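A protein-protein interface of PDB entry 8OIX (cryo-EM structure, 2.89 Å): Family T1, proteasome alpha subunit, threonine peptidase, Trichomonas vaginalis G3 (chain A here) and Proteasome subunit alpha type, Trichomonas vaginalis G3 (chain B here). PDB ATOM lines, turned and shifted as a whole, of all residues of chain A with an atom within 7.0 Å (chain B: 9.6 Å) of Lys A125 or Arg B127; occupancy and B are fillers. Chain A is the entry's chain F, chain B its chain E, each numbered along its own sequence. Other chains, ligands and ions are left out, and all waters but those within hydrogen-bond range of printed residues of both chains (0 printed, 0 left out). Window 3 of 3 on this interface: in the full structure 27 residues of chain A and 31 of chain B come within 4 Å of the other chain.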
ATOM      1  N   ASN A   9       1.642  -7.292 -14.765  1.00  0.00           N
ATOM      2  CA  ASN A   9       0.478  -8.143 -14.585  1.00  0.00           C
ATOM      3  C   ASN A   9      -0.375  -8.097 -15.843  1.00  0.00           C
ATOM      4  O   ASN A   9      -0.235  -7.203 -16.681  1.00  0.00           O
ATOM      5  CB  ASN A   9      -0.362  -7.713 -13.374  1.00  0.00           C
ATOM      6  CG  ASN A   9       0.455  -7.609 -12.102  1.00  0.00           C
ATOM      7  OD1 ASN A   9       0.676  -8.603 -11.409  1.00  0.00           O
ATOM      8  ND2 ASN A   9       0.904  -6.401 -11.785  1.00  0.00           N
ATOM      9  N   ALA A  10      -1.264  -9.082 -15.970  1.00  0.00           N
ATOM     10  CA  ALA A  10      -2.301  -9.009 -16.990  1.00  0.00           C
ATOM     11  C   ALA A  10      -3.316  -7.913 -16.700  1.00  0.00           C
ATOM     12  O   ALA A  10      -4.121  -7.588 -17.578  1.00  0.00           O
ATOM     13  CB  ALA A  10      -3.014 -10.355 -17.114  1.00  0.00           C
ATOM     14  N   THR A  11      -3.288  -7.337 -15.503  1.00  0.00           N
ATOM     15  CA  THR A  11      -4.211  -6.293 -15.087  1.00  0.00           C
ATOM     16  C   THR A  11      -3.667  -4.896 -15.383  1.00  0.00           C
ATOM     17  O   THR A  11      -4.409  -3.912 -15.293  1.00  0.00           O
ATOM     18  CB  THR A  11      -4.511  -6.484 -13.585  1.00  0.00           C
ATOM     19  OG1 THR A  11      -5.325  -7.651 -13.415  1.00  0.00           O
ATOM     20  CG2 THR A  11      -5.246  -5.304 -12.963  1.00  0.00           C
ATOM     21  N   GLN A 115     -13.821 -16.328 -20.234  1.00  0.00           N
ATOM     22  CA  GLN A 115     -12.944 -16.864 -19.200  1.00  0.00           C
ATOM     23  C   GLN A 115     -11.539 -16.285 -19.313  1.00  0.00           C
ATOM     24  O   GLN A 115     -10.936 -15.897 -18.306  1.00  0.00           O
ATOM     25  CB  GLN A 115     -12.908 -18.390 -19.282  1.00  0.00           C
ATOM     26  CG  GLN A 115     -12.021 -19.042 -18.238  1.00  0.00           C
ATOM     27  CD  GLN A 115     -12.790 -19.963 -17.314  1.00  0.00           C
ATOM     28  OE1 GLN A 115     -13.998 -19.814 -17.137  1.00  0.00           O
ATOM     29  NE2 GLN A 115     -12.091 -20.923 -16.720  1.00  0.00           N
ATOM     30  N   LYS A 118     -11.598 -12.709 -18.118  1.00  0.00           N
ATOM     31  CA  LYS A 118     -11.631 -12.669 -16.661  1.00  0.00           C
ATOM     32  C   LYS A 118     -10.276 -13.026 -16.067  1.00  0.00           C
ATOM     33  O   LYS A 118      -9.918 -12.532 -14.993  1.00  0.00           O
ATOM     34  CB  LYS A 118     -12.714 -13.610 -16.133  1.00  0.00           C
ATOM     35  CG  LYS A 118     -14.130 -13.142 -16.423  1.00  0.00           C
ATOM     36  CD  LYS A 118     -15.157 -14.065 -15.793  1.00  0.00           C
ATOM     37  CE  LYS A 118     -15.127 -15.439 -16.436  1.00  0.00           C
ATOM     38  NZ  LYS A 118     -16.212 -16.317 -15.920  1.00  0.00           N
ATOM     39  N   LYS A 119      -9.515 -13.889 -16.744  1.00  0.00           N
ATOM     40  CA  LYS A 119      -8.134 -14.132 -16.337  1.00  0.00           C
ATOM     41  C   LYS A 119      -7.274 -12.887 -16.508  1.00  0.00           C
ATOM     42  O   LYS A 119      -6.366 -12.645 -15.707  1.00  0.00           O
ATOM     43  CB  LYS A 119      -7.540 -15.293 -17.135  1.00  0.00           C
ATOM     44  CG  LYS A 119      -8.208 -16.634 -16.890  1.00  0.00           C
ATOM     45  CD  LYS A 119      -7.880 -17.174 -15.510  1.00  0.00           C
ATOM     46  CE  LYS A 119      -8.280 -18.633 -15.379  1.00  0.00           C
ATOM     47  NZ  LYS A 119      -9.758 -18.808 -15.400  1.00  0.00           N
ATOM     48  N   THR A 120      -7.545 -12.091 -17.538  1.00  0.00           N
ATOM     49  CA  THR A 120      -6.744 -10.901 -17.809  1.00  0.00           C
ATOM     50  C   THR A 120      -7.238  -9.652 -17.087  1.00  0.00           C
ATOM     51  O   THR A 120      -6.561  -8.621 -17.139  1.00  0.00           O
ATOM     52  CB  THR A 120      -6.702 -10.614 -19.314  1.00  0.00           C
ATOM     53  OG1 THR A 120      -8.016 -10.279 -19.775  1.00  0.00           O
ATOM     54  CG2 THR A 120      -6.199 -11.823 -20.071  1.00  0.00           C
ATOM     55  N   SER A 121      -8.394  -9.707 -16.430  1.00  0.00           N
ATOM     56  CA  SER A 121      -8.983  -8.531 -15.803  1.00  0.00           C
ATOM     57  C   SER A 121      -8.843  -8.520 -14.290  1.00  0.00           C
ATOM     58  O   SER A 121      -8.965  -7.453 -13.680  1.00  0.00           O
ATOM     59  CB  SER A 121     -10.468  -8.422 -16.167  1.00  0.00           C
ATOM     60  OG  SER A 121     -11.217  -9.460 -15.561  1.00  0.00           O
ATOM     61  N   LYS A 122      -8.593  -9.671 -13.677  1.00  0.00           N
ATOM     62  CA  LYS A 122      -8.435  -9.798 -12.237  1.00  0.00           C
ATOM     63  C   LYS A 122      -6.985 -10.140 -11.929  1.00  0.00           C
ATOM     64  O   LYS A 122      -6.376 -10.962 -12.622  1.00  0.00           O
ATOM     65  CB  LYS A 122      -9.365 -10.884 -11.689  1.00  0.00           C
ATOM     66  CG  LYS A 122     -10.259 -10.453 -10.539  1.00  0.00           C
ATOM     67  CD  LYS A 122      -9.530 -10.508  -9.209  1.00  0.00           C
ATOM     68  CE  LYS A 122     -10.396  -9.960  -8.088  1.00  0.00           C
ATOM     69  NZ  LYS A 122     -11.701 -10.670  -7.994  1.00  0.00           N
ATOM     70  N   VAL A 123      -6.423  -9.499 -10.900  1.00  0.00           N
ATOM     71  CA  VAL A 123      -5.027  -9.770 -10.580  1.00  0.00           C
ATOM     72  C   VAL A 123      -4.896 -11.183 -10.028  1.00  0.00           C
ATOM     73  O   VAL A 123      -5.865 -11.808  -9.581  1.00  0.00           O
ATOM     74  CB  VAL A 123      -4.446  -8.750  -9.588  1.00  0.00           C
ATOM     75  CG1 VAL A 123      -4.662  -7.334 -10.076  1.00  0.00           C
ATOM     76  CG2 VAL A 123      -5.012  -8.976  -8.198  1.00  0.00           C
ATOM     77  N   GLY A 124      -3.673 -11.689 -10.060  1.00  0.00           N
ATOM     78  CA  GLY A 124      -3.416 -13.024  -9.588  1.00  0.00           C
ATOM     79  C   GLY A 124      -3.794 -14.119 -10.552  1.00  0.00           C
ATOM     80  O   GLY A 124      -3.659 -15.300 -10.209  1.00  0.00           O
ATOM     81  N   LYS A 125      -4.263 -13.770 -11.744  1.00  0.00           N
ATOM     82  CA  LYS A 125      -4.612 -14.733 -12.771  1.00  0.00           C
ATOM     83  C   LYS A 125      -3.777 -14.452 -14.010  1.00  0.00           C
ATOM     84  O   LYS A 125      -3.428 -13.302 -14.295  1.00  0.00           O
ATOM     85  CB  LYS A 125      -6.102 -14.666 -13.116  1.00  0.00           C
ATOM     86  CG  LYS A 125      -7.018 -14.964 -11.945  1.00  0.00           C
ATOM     87  CD  LYS A 125      -8.453 -14.592 -12.255  1.00  0.00           C
ATOM     88  CE  LYS A 125      -9.347 -14.834 -11.055  1.00  0.00           C
ATOM     89  NZ  LYS A 125      -9.265 -16.245 -10.589  1.00  0.00           N
ATOM     90  N   ARG A 126      -3.456 -15.503 -14.732  1.00  0.00           N
ATOM     91  CA  ARG A 126      -2.727 -15.317 -15.967  1.00  0.00           C
ATOM     92  C   ARG A 126      -3.614 -15.654 -17.157  1.00  0.00           C
ATOM     93  O   ARG A 126      -4.482 -16.527 -17.065  1.00  0.00           O
ATOM     94  CB  ARG A 126      -1.472 -16.195 -16.012  1.00  0.00           C
ATOM     95  CG  ARG A 126      -1.764 -17.670 -15.832  1.00  0.00           C
ATOM     96  CD  ARG A 126      -0.646 -18.537 -16.369  1.00  0.00           C
ATOM     97  NE  ARG A 126      -1.107 -19.900 -16.595  1.00  0.00           N
ATOM     98  CZ  ARG A 126      -1.151 -20.839 -15.662  1.00  0.00           C
ATOM     99  NH1 ARG A 126      -0.743 -20.604 -14.425  1.00  0.00           N
ATOM    100  NH2 ARG A 126      -1.623 -22.041 -15.974  1.00  0.00           N
ATOM    101  N   PRO A 127      -3.437 -14.966 -18.282  1.00  0.00           N
ATOM    102  CA  PRO A 127      -4.125 -15.387 -19.505  1.00  0.00           C
ATOM    103  C   PRO A 127      -3.701 -16.794 -19.893  1.00  0.00           C
ATOM    104  O   PRO A 127      -2.549 -17.187 -19.707  1.00  0.00           O
ATOM    105  CB  PRO A 127      -3.675 -14.351 -20.543  1.00  0.00           C
ATOM    106  CG  PRO A 127      -2.451 -13.723 -19.963  1.00  0.00           C
ATOM    107  CD  PRO A 127      -2.631 -13.753 -18.485  1.00  0.00           C
ATOM    108  N   ASN B  11       5.491 -12.051 -10.232  1.00  0.00           N
ATOM    109  CA  ASN B  11       4.402 -12.943  -9.868  1.00  0.00           C
ATOM    110  C   ASN B  11       4.579 -14.284 -10.567  1.00  0.00           C
ATOM    111  O   ASN B  11       5.137 -14.358 -11.663  1.00  0.00           O
ATOM    112  CB  ASN B  11       3.042 -12.333 -10.225  1.00  0.00           C
ATOM    113  CG  ASN B  11       2.918 -12.001 -11.697  1.00  0.00           C
ATOM    114  OD1 ASN B  11       3.578 -11.089 -12.197  1.00  0.00           O
ATOM    115  ND2 ASN B  11       2.065 -12.736 -12.400  1.00  0.00           N
ATOM    116  N   VAL B  12       4.119 -15.350  -9.908  1.00  0.00           N
ATOM    117  CA  VAL B  12       4.417 -16.702 -10.378  1.00  0.00           C
ATOM    118  C   VAL B  12       3.844 -16.932 -11.772  1.00  0.00           C
ATOM    119  O   VAL B  12       4.504 -17.507 -12.647  1.00  0.00           O
ATOM    120  CB  VAL B  12       3.912 -17.756  -9.374  1.00  0.00           C
ATOM    121  CG1 VAL B  12       4.680 -17.650  -8.077  1.00  0.00           C
ATOM    122  CG2 VAL B  12       2.424 -17.615  -9.125  1.00  0.00           C
ATOM    123  N   ASN B  13       2.611 -16.491 -12.004  1.00  0.00           N
ATOM    124  CA  ASN B  13       1.932 -16.745 -13.270  1.00  0.00           C
ATOM    125  C   ASN B  13       2.113 -15.553 -14.209  1.00  0.00           C
ATOM    126  O   ASN B  13       1.172 -14.852 -14.581  1.00  0.00           O
ATOM    127  CB  ASN B  13       0.461 -17.067 -13.021  1.00  0.00           C
ATOM    128  CG  ASN B  13      -0.199 -16.098 -12.059  1.00  0.00           C
ATOM    129  OD1 ASN B  13       0.172 -14.926 -11.981  1.00  0.00           O
ATOM    130  ND2 ASN B  13      -1.181 -16.587 -11.312  1.00  0.00           N
ATOM    131  N   THR B  14       3.368 -15.344 -14.600  1.00  0.00           N
ATOM    132  CA  THR B  14       3.746 -14.266 -15.501  1.00  0.00           C
ATOM    133  C   THR B  14       4.395 -14.860 -16.742  1.00  0.00           C
ATOM    134  O   THR B  14       5.094 -15.876 -16.666  1.00  0.00           O
ATOM    135  CB  THR B  14       4.705 -13.265 -14.832  1.00  0.00           C
ATOM    136  OG1 THR B  14       4.902 -12.142 -15.699  1.00  0.00           O
ATOM    137  CG2 THR B  14       6.056 -13.903 -14.554  1.00  0.00           C
ATOM    138  N   PHE B  15       4.132 -14.243 -17.886  1.00  0.00           N
ATOM    139  CA  PHE B  15       4.678 -14.692 -19.157  1.00  0.00           C
ATOM    140  C   PHE B  15       5.837 -13.791 -19.555  1.00  0.00           C
ATOM    141  O   PHE B  15       5.718 -12.563 -19.515  1.00  0.00           O
ATOM    142  CB  PHE B  15       3.605 -14.684 -20.246  1.00  0.00           C
ATOM    143  CG  PHE B  15       2.615 -15.803 -20.132  1.00  0.00           C
ATOM    144  CD1 PHE B  15       2.901 -17.053 -20.652  1.00  0.00           C
ATOM    145  CD2 PHE B  15       1.394 -15.603 -19.515  1.00  0.00           C
ATOM    146  CE1 PHE B  15       1.990 -18.083 -20.555  1.00  0.00           C
ATOM    147  CE2 PHE B  15       0.481 -16.630 -19.412  1.00  0.00           C
ATOM    148  CZ  PHE B  15       0.778 -17.872 -19.933  1.00  0.00           C
ATOM    149  N   LEU B  21       6.029 -19.133 -19.461  1.00  0.00           N
ATOM    150  CA  LEU B  21       5.744 -18.990 -18.038  1.00  0.00           C
ATOM    151  C   LEU B  21       7.054 -19.106 -17.269  1.00  0.00           C
ATOM    152  O   LEU B  21       7.656 -20.182 -17.221  1.00  0.00           O
ATOM    153  CB  LEU B  21       4.743 -20.047 -17.584  1.00  0.00           C
ATOM    154  CG  LEU B  21       3.264 -19.661 -17.586  1.00  0.00           C
ATOM    155  CD1 LEU B  21       2.413 -20.827 -17.119  1.00  0.00           C
ATOM    156  CD2 LEU B  21       3.032 -18.446 -16.710  1.00  0.00           C
ATOM    157  N   PHE B 123      -1.139 -23.900 -10.324  1.00  0.00           N
ATOM    158  CA  PHE B 123      -0.530 -23.010  -9.348  1.00  0.00           C
ATOM    159  C   PHE B 123      -0.983 -21.573  -9.560  1.00  0.00           C
ATOM    160  O   PHE B 123      -1.219 -21.130 -10.688  1.00  0.00           O
ATOM    161  CB  PHE B 123       0.997 -23.105  -9.413  1.00  0.00           C
ATOM    162  CG  PHE B 123       1.601 -22.483 -10.641  1.00  0.00           C
ATOM    163  CD1 PHE B 123       1.748 -23.219 -11.803  1.00  0.00           C
ATOM    164  CD2 PHE B 123       2.050 -21.172 -10.624  1.00  0.00           C
ATOM    165  CE1 PHE B 123       2.311 -22.654 -12.929  1.00  0.00           C
ATOM    166  CE2 PHE B 123       2.613 -20.604 -11.747  1.00  0.00           C
ATOM    167  CZ  PHE B 123       2.744 -21.346 -12.901  1.00  0.00           C
ATOM    168  N   GLY B 124      -1.103 -20.842  -8.456  1.00  0.00           N
ATOM    169  CA  GLY B 124      -1.575 -19.472  -8.521  1.00  0.00           C
ATOM    170  C   GLY B 124      -1.159 -18.669  -7.312  1.00  0.00           C
ATOM    171  O   GLY B 124      -0.820 -19.212  -6.257  1.00  0.00           O
ATOM    172  N   GLU B 125      -1.192 -17.351  -7.490  1.00  0.00           N
ATOM    173  CA  GLU B 125      -0.808 -16.383  -6.474  1.00  0.00           C
ATOM    174  C   GLU B 125      -1.704 -15.168  -6.642  1.00  0.00           C
ATOM    175  O   GLU B 125      -2.217 -14.914  -7.730  1.00  0.00           O
ATOM    176  CB  GLU B 125       0.671 -16.000  -6.618  1.00  0.00           C
ATOM    177  CG  GLU B 125       1.134 -14.780  -5.844  1.00  0.00           C
ATOM    178  CD  GLU B 125       2.553 -14.387  -6.200  1.00  0.00           C
ATOM    179  OE1 GLU B 125       2.977 -14.670  -7.340  1.00  0.00           O
ATOM    180  OE2 GLU B 125       3.239 -13.775  -5.358  1.00  0.00           O
ATOM    181  N   GLY B 126      -1.909 -14.426  -5.556  1.00  0.00           N
ATOM    182  CA  GLY B 126      -2.606 -13.161  -5.634  1.00  0.00           C
ATOM    183  C   GLY B 126      -4.109 -13.231  -5.473  1.00  0.00           C
ATOM    184  O   GLY B 126      -4.755 -12.179  -5.397  1.00  0.00           O
ATOM    185  N   ARG B 127      -4.692 -14.425  -5.450  1.00  0.00           N
ATOM    186  CA  ARG B 127      -6.125 -14.593  -5.265  1.00  0.00           C
ATOM    187  C   ARG B 127      -6.405 -15.184  -3.891  1.00  0.00           C
ATOM    188  O   ARG B 127      -5.652 -16.037  -3.407  1.00  0.00           O
ATOM    189  CB  ARG B 127      -6.725 -15.488  -6.352  1.00  0.00           C
ATOM    190  CG  ARG B 127      -7.427 -14.732  -7.473  1.00  0.00           C
ATOM    191  CD  ARG B 127      -8.576 -13.867  -6.960  1.00  0.00           C
ATOM    192  NE  ARG B 127      -9.282 -14.467  -5.832  1.00  0.00           N
ATOM    193  CZ  ARG B 127     -10.192 -15.426  -5.936  1.00  0.00           C
ATOM    194  NH1 ARG B 127     -10.529 -15.936  -7.109  1.00  0.00           N
ATOM    195  NH2 ARG B 127     -10.777 -15.887  -4.834  1.00  0.00           N
ATOM    196  N   ARG B 128      -7.486 -14.722  -3.269  1.00  0.00           N
ATOM    197  CA  ARG B 128      -7.862 -15.208  -1.948  1.00  0.00           C
ATOM    198  C   ARG B 128      -8.129 -16.708  -1.984  1.00  0.00           C
ATOM    199  O   ARG B 128      -8.640 -17.240  -2.973  1.00  0.00           O
ATOM    200  CB  ARG B 128      -9.097 -14.462  -1.446  1.00  0.00           C
ATOM    201  CG  ARG B 128      -9.017 -12.951  -1.602  1.00  0.00           C
ATOM    202  CD  ARG B 128      -7.789 -12.388  -0.906  1.00  0.00           C
ATOM    203  NE  ARG B 128      -8.141 -11.412   0.119  1.00  0.00           N
ATOM    204  CZ  ARG B 128      -8.326 -10.120  -0.109  1.00  0.00           C
ATOM    205  NH1 ARG B 128      -8.213  -9.610  -1.325  1.00  0.00           N
ATOM    206  NH2 ARG B 128      -8.633  -9.319   0.906  1.00  0.00           N
ATOM    207  N   LYS B 129      -7.762 -17.388  -0.901  1.00  0.00           N
ATOM    208  CA  LYS B 129      -7.892 -18.840  -0.797  1.00  0.00           C
ATOM    209  C   LYS B 129      -9.308 -19.320  -1.103  1.00  0.00           C
ATOM    210  O   LYS B 129     -10.281 -18.805  -0.551  1.00  0.00           O
ATOM    211  CB  LYS B 129      -7.477 -19.309   0.599  1.00  0.00           C
ATOM    212  CG  LYS B 129      -6.053 -18.943   0.974  1.00  0.00           C
ATOM    213  CD  LYS B 129      -5.717 -19.375   2.389  1.00  0.00           C
ATOM    214  CE  LYS B 129      -4.408 -18.757   2.853  1.00  0.00           C
ATOM    215  NZ  LYS B 129      -4.159 -19.007   4.299  1.00  0.00           N
ATOM    216  N   GLN B 134      -4.886 -23.945  -2.897  1.00  0.00           N
ATOM    217  CA  GLN B 134      -4.184 -23.929  -4.173  1.00  0.00           C
ATOM    218  C   GLN B 134      -2.674 -23.843  -3.977  1.00  0.00           C
ATOM    219  O   GLN B 134      -2.192 -23.145  -3.085  1.00  0.00           O
ATOM    220  CB  GLN B 134      -4.661 -22.757  -5.033  1.00  0.00           C
ATOM    221  CG  GLN B 134      -4.122 -22.773  -6.452  1.00  0.00           C
ATOM    222  CD  GLN B 134      -4.373 -21.475  -7.191  1.00  0.00           C
ATOM    223  OE1 GLN B 134      -4.263 -20.391  -6.621  1.00  0.00           O
ATOM    224  NE2 GLN B 134      -4.710 -21.581  -8.473  1.00  0.00           N
ATOM    225  N   MET B 135      -1.934 -24.558  -4.818  1.00  0.00           N
ATOM    226  CA  MET B 135      -0.482 -24.475  -4.797  1.00  0.00           C
ATOM    227  C   MET B 135      -0.020 -23.124  -5.334  1.00  0.00           C
ATOM    228  O   MET B 135      -0.665 -22.514  -6.189  1.00  0.00           O
ATOM    229  CB  MET B 135       0.116 -25.622  -5.614  1.00  0.00           C
ATOM    230  CG  MET B 135      -0.393 -25.674  -7.043  1.00  0.00           C
ATOM    231  SD  MET B 135      -0.148 -27.262  -7.861  1.00  0.00           S
ATOM    232  CE  MET B 135       1.548 -27.118  -8.405  1.00  0.00           C
ATOM    233  N   SER B 136       1.107 -22.647  -4.805  1.00  0.00           N
ATOM    234  CA  SER B 136       1.601 -21.312  -5.114  1.00  0.00           C
ATOM    235  C   SER B 136       2.675 -21.294  -6.192  1.00  0.00           C
ATOM    236  O   SER B 136       3.070 -20.210  -6.630  1.00  0.00           O
ATOM    237  CB  SER B 136       2.150 -20.645  -3.848  1.00  0.00           C
ATOM    238  OG  SER B 136       3.322 -21.296  -3.393  1.00  0.00           O
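O of Glu B125 sits close to O of Gly A124, 2.9 Å away.
The backbone carbonyl oxygen (O) of Gly A124 lies within hydrogen-bond range of the side-chain amide nitrogen (ND2) of Asn B13, at 3.0 Å.
The side-chain hydroxyl (OG1) of Thr A11 sits at hydrogen-bond distance from the backbone NH (N) of Val A123 (3.3 Å).
The side-chain amide nitrogen of Asn B11 is in hydrogen-bond range of the side-chain amide oxygen of Asn B13.
The backbone NH of Val B12 is in hydrogen-bond range of the side-chain carboxylate of Glu B125 (2.9 Å).
Printed residues of chain B that touch a printed residue of chain A: Asn B11, Asn B13, Phe B15, Leu B21, Phe B123, Glu B125 and Arg B127.
Hydrophobic or aromatic side chains of chain B within 4 Å of the printed part of chain A: Phe B15, Leu B21 and Phe B123.
Of the 14 printed residues of chain A, 6 touch a printed residue of chain B.
Among the printed residues, pairs that only touch across the chains: Asn A9 with Asn B11 (3.9 Å), Val A123 with Arg B127 (3.9 Å), Lys A125 with Arg B127 (3.7 Å), Arg A126 with Asn B13 (3.3 Å), Arg A126 with Phe B15 (3.8 Å), Arg A126 with Leu B21 (3.7 Å), Arg A126 with Phe B123 (3.8 Å) and Pro A127 with Phe B15 (3.1 Å).
Of the printed residues of chain B, Asn A9 touches Asn B11 (3.9 Å).
No residue of chain B comes within 4 Å of Lys A119.
Thr A120 touches none of the printed residues of chain B.
Of the printed residues of chain B, Gly A124 touches Asn B13 and Glu B125.
Lys A125 touches just one residue of chain B: Arg B127 (3.7 Å).
Of the printed residues of chain A, Asn B11 touches Asn A9 (3.9 Å).
Of the printed residues of chain A, Asn B13 touches Gly A124 and Arg A126.
Gly B126 touches none of the printed residues of chain A.
Arg B127 touches just these residues of chain A: Val A123 and Lys A125.
Met B135 touches none of the printed residues of chain A.
The nearest residue of chain A that does not touch Arg B127 is Lys A122 (4.2 Å).
The nearest printed residue of chain B that does not touch Pro A127 is Asn B13 (5.6 Å).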
